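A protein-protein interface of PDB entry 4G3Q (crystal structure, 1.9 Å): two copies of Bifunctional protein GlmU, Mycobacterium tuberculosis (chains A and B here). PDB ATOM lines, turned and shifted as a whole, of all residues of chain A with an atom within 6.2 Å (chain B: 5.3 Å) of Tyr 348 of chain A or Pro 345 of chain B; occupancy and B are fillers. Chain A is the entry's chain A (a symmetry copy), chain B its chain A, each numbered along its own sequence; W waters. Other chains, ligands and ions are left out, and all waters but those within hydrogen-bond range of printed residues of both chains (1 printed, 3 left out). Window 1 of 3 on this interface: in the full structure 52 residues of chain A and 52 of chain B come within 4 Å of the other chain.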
ATOM      1  N   ARG A 329      -4.964 -26.842  -2.002  1.00  0.00           N
ATOM      2  CA  ARG A 329      -4.576 -26.882  -3.473  1.00  0.00           C
ATOM      3  C   ARG A 329      -5.752 -26.517  -4.365  1.00  0.00           C
ATOM      4  O   ARG A 329      -6.118 -27.243  -5.281  1.00  0.00           O
ATOM      5  CB  ARG A 329      -4.042 -28.269  -3.820  1.00  0.00           C
ATOM      6  CG  ARG A 329      -2.708 -28.592  -3.123  1.00  0.00           C
ATOM      7  CD  ARG A 329      -1.930 -29.803  -3.877  1.00  0.00           C
ATOM      8  NE  ARG A 329      -0.658 -29.901  -3.182  1.00  0.00           N
ATOM      9  CZ  ARG A 329       0.405 -29.225  -3.564  1.00  0.00           C
ATOM     10  NH1 ARG A 329       0.340 -28.489  -4.695  1.00  0.00           N
ATOM     11  NH2 ARG A 329       1.502 -29.260  -2.812  1.00  0.00           N
ATOM     12  N   THR A 330      -6.371 -25.369  -4.076  1.00  0.00           N
ATOM     13  CA  THR A 330      -7.614 -24.999  -4.768  1.00  0.00           C
ATOM     14  C   THR A 330      -7.333 -23.660  -5.456  1.00  0.00           C
ATOM     15  O   THR A 330      -6.634 -22.812  -4.902  1.00  0.00           O
ATOM     16  CB  THR A 330      -8.768 -24.860  -3.707  1.00  0.00           C
ATOM     17  OG1 THR A 330      -9.104 -26.190  -3.277  1.00  0.00           O
ATOM     18  CG2 THR A 330     -10.089 -24.251  -4.274  1.00  0.00           C
ATOM     19  N   HIS A 331      -7.888 -23.482  -6.652  1.00  0.00           N
ATOM     20  CA  HIS A 331      -7.770 -22.216  -7.348  1.00  0.00           C
ATOM     21  C   HIS A 331      -9.226 -21.709  -7.484  1.00  0.00           C
ATOM     22  O   HIS A 331     -10.042 -22.404  -8.110  1.00  0.00           O
ATOM     23  CB  HIS A 331      -7.223 -22.483  -8.775  1.00  0.00           C
ATOM     24  CG  HIS A 331      -6.685 -21.232  -9.432  1.00  0.00           C
ATOM     25  ND1 HIS A 331      -5.460 -20.672  -9.095  1.00  0.00           N
ATOM     26  CD2 HIS A 331      -7.248 -20.398 -10.340  1.00  0.00           C
ATOM     27  CE1 HIS A 331      -5.315 -19.534  -9.764  1.00  0.00           C
ATOM     28  NE2 HIS A 331      -6.360 -19.373 -10.557  1.00  0.00           N
ATOM     29  N   GLY A 332      -9.564 -20.549  -6.944  1.00  0.00           N
ATOM     30  CA  GLY A 332     -11.037 -20.300  -6.826  1.00  0.00           C
ATOM     31  C   GLY A 332     -11.323 -18.798  -6.854  1.00  0.00           C
ATOM     32  O   GLY A 332     -10.493 -17.998  -6.393  1.00  0.00           O
ATOM     33  N   SER A 333     -12.459 -18.397  -7.406  1.00  0.00           N
ATOM     34  CA  SER A 333     -12.832 -17.017  -7.318  1.00  0.00           C
ATOM     35  C   SER A 333     -14.344 -16.886  -7.224  1.00  0.00           C
ATOM     36  O   SER A 333     -15.092 -17.727  -7.722  1.00  0.00           O
ATOM     37  CB  SER A 333     -12.274 -16.169  -8.467  1.00  0.00           C
ATOM     38  OG  SER A 333     -12.891 -16.453  -9.706  1.00  0.00           O
ATOM     39  N   PHE A 346      -6.523 -29.953  -5.714  1.00  0.00           N
ATOM     40  CA  PHE A 346      -6.665 -29.863  -7.198  1.00  0.00           C
ATOM     41  C   PHE A 346      -8.128 -29.643  -7.595  1.00  0.00           C
ATOM     42  O   PHE A 346      -8.733 -30.427  -8.367  1.00  0.00           O
ATOM     43  CB  PHE A 346      -6.091 -31.053  -7.980  1.00  0.00           C
ATOM     44  CG  PHE A 346      -4.711 -31.471  -7.540  1.00  0.00           C
ATOM     45  CD1 PHE A 346      -3.580 -30.690  -7.851  1.00  0.00           C
ATOM     46  CD2 PHE A 346      -4.542 -32.695  -6.857  1.00  0.00           C
ATOM     47  CE1 PHE A 346      -2.263 -31.089  -7.460  1.00  0.00           C
ATOM     48  CE2 PHE A 346      -3.203 -33.115  -6.477  1.00  0.00           C
ATOM     49  CZ  PHE A 346      -2.114 -32.324  -6.788  1.00  0.00           C
ATOM     50  N   THR A 347      -8.648 -28.511  -7.135  1.00  0.00           N
ATOM     51  CA  THR A 347     -10.040 -28.206  -7.384  1.00  0.00           C
ATOM     52  C   THR A 347     -10.114 -26.754  -7.921  1.00  0.00           C
ATOM     53  O   THR A 347      -9.394 -25.905  -7.429  1.00  0.00           O
ATOM     54  CB  THR A 347     -10.857 -28.319  -6.085  1.00  0.00           C
ATOM     55  OG1 THR A 347     -10.687 -29.647  -5.543  1.00  0.00           O
ATOM     56  CG2 THR A 347     -12.400 -28.069  -6.422  1.00  0.00           C
ATOM     57  N   TYR A 348     -10.953 -26.526  -8.932  1.00  0.00           N
ATOM     58  CA  TYR A 348     -11.088 -25.200  -9.581  1.00  0.00           C
ATOM     59  C   TYR A 348     -12.484 -24.684  -9.359  1.00  0.00           C
ATOM     60  O   TYR A 348     -13.442 -25.357  -9.825  1.00  0.00           O
ATOM     61  CB  TYR A 348     -10.904 -25.445 -11.092  1.00  0.00           C
ATOM     62  CG  TYR A 348     -10.893 -24.168 -11.938  1.00  0.00           C
ATOM     63  CD1 TYR A 348     -10.593 -22.904 -11.393  1.00  0.00           C
ATOM     64  CD2 TYR A 348     -11.133 -24.276 -13.299  1.00  0.00           C
ATOM     65  CE1 TYR A 348     -10.576 -21.685 -12.276  1.00  0.00           C
ATOM     66  CE2 TYR A 348     -11.126 -23.151 -14.134  1.00  0.00           C
ATOM     67  CZ  TYR A 348     -10.864 -21.905 -13.595  1.00  0.00           C
ATOM     68  OH  TYR A 348     -10.898 -20.860 -14.475  1.00  0.00           O
ATOM     69  N   LEU A 349     -12.644 -23.517  -8.673  1.00  0.00           N
ATOM     70  CA  LEU A 349     -13.985 -22.933  -8.447  1.00  0.00           C
ATOM     71  C   LEU A 349     -14.086 -21.659  -9.305  1.00  0.00           C
ATOM     72  O   LEU A 349     -13.243 -20.784  -9.196  1.00  0.00           O
ATOM     73  CB  LEU A 349     -14.186 -22.499  -6.994  1.00  0.00           C
ATOM     74  CG  LEU A 349     -13.913 -23.579  -5.936  1.00  0.00           C
ATOM     75  CD1 LEU A 349     -14.305 -23.214  -4.503  1.00  0.00           C
ATOM     76  CD2 LEU A 349     -14.692 -24.891  -6.347  1.00  0.00           C
ATOM     77  N   ARG A 350     -15.010 -21.650 -10.241  1.00  0.00           N
ATOM     78  CA  ARG A 350     -15.238 -20.431 -11.060  1.00  0.00           C
ATOM     79  C   ARG A 350     -16.388 -19.677 -10.475  1.00  0.00           C
ATOM     80  O   ARG A 350     -17.121 -20.219  -9.645  1.00  0.00           O
ATOM     81  CB  ARG A 350     -15.550 -20.827 -12.514  1.00  0.00           C
ATOM     82  CG  ARG A 350     -14.217 -21.386 -13.220  1.00  0.00           C
ATOM     83  CD  ARG A 350     -14.527 -22.100 -14.515  1.00  0.00           C
ATOM     84  NE  ARG A 350     -15.156 -21.276 -15.531  1.00  0.00           N
ATOM     85  CZ  ARG A 350     -15.882 -21.783 -16.539  1.00  0.00           C
ATOM     86  NH1 ARG A 350     -16.099 -23.109 -16.615  1.00  0.00           N
ATOM     87  NH2 ARG A 350     -16.437 -20.965 -17.440  1.00  0.00           N
ATOM     88  N   THR A 353     -19.911 -20.225  -7.806  1.00  0.00           N
ATOM     89  CA  THR A 353     -19.980 -21.526  -7.130  1.00  0.00           C
ATOM     90  C   THR A 353     -20.419 -21.295  -5.673  1.00  0.00           C
ATOM     91  O   THR A 353     -19.856 -20.428  -5.007  1.00  0.00           O
ATOM     92  CB  THR A 353     -18.602 -22.247  -7.163  1.00  0.00           C
ATOM     93  OG1 THR A 353     -18.299 -22.533  -8.530  1.00  0.00           O
ATOM     94  CG2 THR A 353     -18.650 -23.543  -6.375  1.00  0.00           C
ATOM     95  N   GLY A 362     -13.943 -32.602  -4.609  1.00  0.00           N
ATOM     96  CA  GLY A 362     -12.645 -33.266  -4.495  1.00  0.00           C
ATOM     97  C   GLY A 362     -11.727 -33.008  -5.663  1.00  0.00           C
ATOM     98  O   GLY A 362     -11.784 -31.958  -6.332  1.00  0.00           O
ATOM     99  N   VAL A 365     -11.918 -31.656  -9.806  1.00  0.00           N
ATOM    100  CA  VAL A 365     -13.309 -31.215  -9.957  1.00  0.00           C
ATOM    101  C   VAL A 365     -13.255 -29.711 -10.280  1.00  0.00           C
ATOM    102  O   VAL A 365     -12.473 -28.965  -9.693  1.00  0.00           O
ATOM    103  CB  VAL A 365     -14.120 -31.503  -8.612  1.00  0.00           C
ATOM    104  CG1 VAL A 365     -15.543 -30.758  -8.603  1.00  0.00           C
ATOM    105  CG2 VAL A 365     -14.294 -33.007  -8.475  1.00  0.00           C
ATOM    106  N   GLU A 366     -14.107 -29.300 -11.216  1.00  0.00           N
ATOM    107  CA  GLU A 366     -14.267 -27.890 -11.563  1.00  0.00           C
ATOM    108  C   GLU A 366     -15.761 -27.608 -11.400  1.00  0.00           C
ATOM    109  O   GLU A 366     -16.596 -28.365 -11.952  1.00  0.00           O
ATOM    110  CB  GLU A 366     -13.916 -27.672 -13.041  1.00  0.00           C
ATOM    111  CG  GLU A 366     -14.267 -26.225 -13.477  1.00  0.00           C
ATOM    112  CD  GLU A 366     -13.795 -25.892 -14.911  1.00  0.00           C
ATOM    113  OE1 GLU A 366     -12.781 -26.480 -15.396  1.00  0.00           O
ATOM    114  OE2 GLU A 366     -14.387 -25.022 -15.525  1.00  0.00           O
ATOM    115  N   VAL A 367     -16.099 -26.493 -10.750  1.00  0.00           N
ATOM    116  CA  VAL A 367     -17.542 -26.041 -10.642  1.00  0.00           C
ATOM    117  C   VAL A 367     -17.610 -24.578 -11.121  1.00  0.00           C
ATOM    118  O   VAL A 367     -16.691 -23.792 -10.866  1.00  0.00           O
ATOM    119  CB  VAL A 367     -18.047 -26.141  -9.216  1.00  0.00           C
ATOM    120  CG1 VAL A 367     -19.578 -25.705  -9.098  1.00  0.00           C
ATOM    121  CG2 VAL A 367     -17.871 -27.625  -8.728  1.00  0.00           C
ATOM    122  N   LYS A 368     -18.692 -24.252 -11.827  1.00  0.00           N
ATOM    123  CA  LYS A 368     -18.930 -22.923 -12.356  1.00  0.00           C
ATOM    124  C   LYS A 368     -20.412 -22.642 -12.177  1.00  0.00           C
ATOM    125  O   LYS A 368     -21.246 -23.472 -12.609  1.00  0.00           O
ATOM    126  CB  LYS A 368     -18.631 -22.985 -13.852  1.00  0.00           C
ATOM    127  CG  LYS A 368     -18.883 -21.646 -14.615  1.00  0.00           C
ATOM    128  CD  LYS A 368     -20.076 -21.859 -15.650  1.00  0.00           C
ATOM    129  CE  LYS A 368     -20.529 -20.542 -16.371  1.00  0.00           C
ATOM    130  NZ  LYS A 368     -21.392 -20.977 -17.587  1.00  0.00           N
ATOM    131  N   VAL B 328      -1.569 -20.460 -16.390  1.00  0.00           N
ATOM    132  CA  VAL B 328      -1.785 -20.397 -14.963  1.00  0.00           C
ATOM    133  C   VAL B 328      -1.759 -21.834 -14.412  1.00  0.00           C
ATOM    134  O   VAL B 328      -2.352 -22.728 -15.032  1.00  0.00           O
ATOM    135  CB  VAL B 328      -3.172 -19.790 -14.711  1.00  0.00           C
ATOM    136  CG1 VAL B 328      -3.554 -19.943 -13.198  1.00  0.00           C
ATOM    137  CG2 VAL B 328      -3.188 -18.313 -15.191  1.00  0.00           C
ATOM    138  N   ARG B 329      -1.072 -22.047 -13.274  1.00  0.00           N
ATOM    139  CA  ARG B 329      -1.000 -23.435 -12.654  1.00  0.00           C
ATOM    140  C   ARG B 329      -0.781 -24.503 -13.712  1.00  0.00           C
ATOM    141  O   ARG B 329      -1.518 -25.477 -13.811  1.00  0.00           O
ATOM    142  CB  ARG B 329      -2.278 -23.707 -11.866  1.00  0.00           C
ATOM    143  CG  ARG B 329      -2.426 -22.804 -10.628  1.00  0.00           C
ATOM    144  CD  ARG B 329      -3.479 -23.434  -9.564  1.00  0.00           C
ATOM    145  NE  ARG B 329      -3.412 -22.541  -8.420  1.00  0.00           N
ATOM    146  CZ  ARG B 329      -2.573 -22.734  -7.425  1.00  0.00           C
ATOM    147  NH1 ARG B 329      -1.813 -23.852  -7.418  1.00  0.00           N
ATOM    148  NH2 ARG B 329      -2.473 -21.812  -6.470  1.00  0.00           N
ATOM    149  N   VAL B 343      -4.304 -21.056 -20.885  1.00  0.00           N
ATOM    150  CA  VAL B 343      -3.906 -22.399 -20.482  1.00  0.00           C
ATOM    151  C   VAL B 343      -4.040 -22.416 -18.924  1.00  0.00           C
ATOM    152  O   VAL B 343      -3.582 -21.472 -18.247  1.00  0.00           O
ATOM    153  CB  VAL B 343      -2.436 -22.728 -20.927  1.00  0.00           C
ATOM    154  CG1 VAL B 343      -2.034 -24.148 -20.420  1.00  0.00           C
ATOM    155  CG2 VAL B 343      -2.355 -22.660 -22.500  1.00  0.00           C
ATOM    156  N   GLY B 344      -4.656 -23.481 -18.378  1.00  0.00           N
ATOM    157  CA  GLY B 344      -4.768 -23.645 -16.934  1.00  0.00           C
ATOM    158  C   GLY B 344      -6.139 -23.246 -16.390  1.00  0.00           C
ATOM    159  O   GLY B 344      -7.027 -22.883 -17.167  1.00  0.00           O
ATOM    160  N   PRO B 345      -6.357 -23.361 -15.055  1.00  0.00           N
ATOM    161  CA  PRO B 345      -5.410 -23.849 -14.091  1.00  0.00           C
ATOM    162  C   PRO B 345      -5.357 -25.409 -14.130  1.00  0.00           C
ATOM    163  O   PRO B 345      -6.301 -26.044 -14.570  1.00  0.00           O
ATOM    164  CB  PRO B 345      -5.986 -23.376 -12.734  1.00  0.00           C
ATOM    165  CG  PRO B 345      -7.535 -23.459 -12.969  1.00  0.00           C
ATOM    166  CD  PRO B 345      -7.697 -23.081 -14.485  1.00  0.00           C
ATOM    167  N   PHE B 346      -4.240 -26.003 -13.724  1.00  0.00           N
ATOM    168  CA  PHE B 346      -4.117 -27.490 -13.638  1.00  0.00           C
ATOM    169  C   PHE B 346      -4.103 -28.119 -15.034  1.00  0.00           C
ATOM    170  O   PHE B 346      -4.939 -28.990 -15.379  1.00  0.00           O
ATOM    171  CB  PHE B 346      -5.180 -28.181 -12.771  1.00  0.00           C
ATOM    172  CG  PHE B 346      -5.404 -27.526 -11.432  1.00  0.00           C
ATOM    173  CD1 PHE B 346      -4.452 -27.636 -10.398  1.00  0.00           C
ATOM    174  CD2 PHE B 346      -6.614 -26.839 -11.190  1.00  0.00           C
ATOM    175  CE1 PHE B 346      -4.666 -27.039  -9.116  1.00  0.00           C
ATOM    176  CE2 PHE B 346      -6.844 -26.249  -9.882  1.00  0.00           C
ATOM    177  CZ  PHE B 346      -5.889 -26.367  -8.890  1.00  0.00           C
ATOM    178  N   THR B 347      -3.078 -27.737 -15.787  1.00  0.00           N
ATOM    179  CA  THR B 347      -2.973 -28.208 -17.151  1.00  0.00           C
ATOM    180  C   THR B 347      -1.530 -28.732 -17.359  1.00  0.00           C
ATOM    181  O   THR B 347      -0.602 -28.117 -16.865  1.00  0.00           O
ATOM    182  CB  THR B 347      -3.255 -27.063 -18.139  1.00  0.00           C
ATOM    183  OG1 THR B 347      -4.562 -26.517 -17.859  1.00  0.00           O
ATOM    184  CG2 THR B 347      -3.224 -27.646 -19.629  1.00  0.00           C
ATOM    185  N   GLY B 362      -8.000 -26.167 -20.733  1.00  0.00           N
ATOM    186  CA  GLY B 362      -8.468 -25.850 -19.385  1.00  0.00           C
ATOM    187  C   GLY B 362      -8.033 -26.848 -18.342  1.00  0.00           C
ATOM    188  O   GLY B 362      -6.980 -27.503 -18.449  1.00  0.00           O
ATOM    189  N   ALA B 363      -8.818 -26.880 -17.259  1.00  0.00           N
ATOM    190  CA  ALA B 363      -8.434 -27.614 -16.094  1.00  0.00           C
ATOM    191  C   ALA B 363      -8.520 -29.082 -16.319  1.00  0.00           C
ATOM    192  O   ALA B 363      -9.550 -29.577 -16.819  1.00  0.00           O
ATOM    193  CB  ALA B 363      -9.365 -27.175 -14.904  1.00  0.00           C
ATOM    194  N   PHE B 364      -7.465 -29.804 -15.858  1.00  0.00           N
ATOM    195  CA  PHE B 364      -7.403 -31.255 -15.829  1.00  0.00           C
ATOM    196  C   PHE B 364      -7.322 -31.731 -17.291  1.00  0.00           C
ATOM    197  O   PHE B 364      -7.885 -32.728 -17.697  1.00  0.00           O
ATOM    198  CB  PHE B 364      -8.528 -31.888 -14.980  1.00  0.00           C
ATOM    199  CG  PHE B 364      -8.836 -31.076 -13.750  1.00  0.00           C
ATOM    200  CD1 PHE B 364      -7.823 -30.772 -12.827  1.00  0.00           C
ATOM    201  CD2 PHE B 364     -10.121 -30.605 -13.545  1.00  0.00           C
ATOM    202  CE1 PHE B 364      -8.106 -30.001 -11.693  1.00  0.00           C
ATOM    203  CE2 PHE B 364     -10.422 -29.797 -12.445  1.00  0.00           C
ATOM    204  CZ  PHE B 364      -9.408 -29.467 -11.502  1.00  0.00           C
HETATM  205  O   HOH W   1     -12.240 -29.225 -15.870  1.00  0.00           O
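The backbone carbonyl oxygen (O) of Arg 329 of chain B sits at hydrogen-bond distance from the backbone NH (N) of Phe 346 of chain B (2.8 Å).
The backbone carbonyl oxygen of Thr 347 of chain A sits at hydrogen-bond distance from the backbone NH of His 331 of chain A (3.0 Å).
The backbone NH (N) of Val 328 of chain B lies within hydrogen-bond range of the backbone carbonyl oxygen (O) of Val 343 of chain B (2.9 Å).
OG1 of Thr 347 of chain A is in hydrogen-bond range of O of Gly 362 of chain A, 2.7 Å away.
O of Phe 346 of chain B sits at hydrogen-bond distance from N of Phe 364 of chain B, 2.7 Å away.
The backbone carbonyl oxygen of Arg 329 of chain A is in hydrogen-bond range of the backbone NH of Phe 346 of chain A, 2.8 Å away.
A ring nitrogen (ND1) of His 331 of chain A lies within hydrogen-bond range of the guanidinium group (NE) of Arg 329 of chain B (2.9 Å).
Of the printed residues of chain B, Arg 329 of chain A touches Phe 346.
Of chain B, only Pro 345 (3.4 Å) and Ala 363 (3.8 Å) come within 4 Å of Tyr 348 of chain A.
Printed residues of chain B within 4 Å of Glu 366 of chain A: Ala 363 and Phe 364.
Printed residues of chain A within 4 Å of Val 328 of chain B: His 331 (3.9 Å).
Gly 344 of chain B touches none of the printed residues of chain A.
The nearest printed residue of chain A that does not touch Pro 345 of chain B is Glu 366 of chain A (6.2 Å).
Arg 329 of chain A touches Phe 346 of chain B, but with the chains exchanged Phe 346 of chain A does not touch Arg 329 of chain B (7.1 Å).
Phe 346 of chain B touches its own counterpart, Phe 346 of chain A.
Thr 347 of chain A touches Phe 346 of chain B, but with the chains exchanged Phe 346 of chain A does not touch Thr 347 of chain B (8.5 Å).
Positions printed for both chains: 329, 346, 347 and 362.
Of the 13 pairs that touch across the chains among the printed residues, 1 has its exchanged pair printed and touching as well.
Water W1 lies within hydrogen-bond range of the side-chain carboxylate of Glu 366 of chain A (2.8 Å) and the backbone carbonyl oxygen of Ala 363 of chain B (2.9 Å).
Phe 346 of chain B touches Arg 329 of chain A (CZ to O, 3.7 Å).
CE1 of His 331 of chain A touches CG1 of Val 328 of chain B (3.9 Å).
CB of His 331 of chain A touches CE2 of Phe 346 of chain B, at 3.9 Å.
Phe 346 of chain B touches Phe 346 of chain A (CE1 to CA, 3.96 Å).
Phe 364 of chain B touches Phe 346 of chain A (CZ to O, 3.3 Å).
O of Thr 347 of chain A touches CE2 of Phe 346 of chain B (3.6 Å).
Tyr 348 of chain A touches Pro 345 of chain B (CE2 to CD, 3.4 Å).
Tyr 348 of chain A touches Ala 363 of chain B (CD2 to CB, 3.8 Å).
Val 365 of chain A touches Phe 364 of chain B (O to CE2, 3.5 Å).
Glu 366 of chain A touches Phe 364 of chain B.
Hydrophobic or aromatic side chains of chain B that line the printed part of chain A: Val 328, Pro 345, Phe 346, Ala 363 and Phe 364.
Hydrophobic or aromatic side chains of chain A that line the printed part of chain B: His 331 and Tyr 348.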
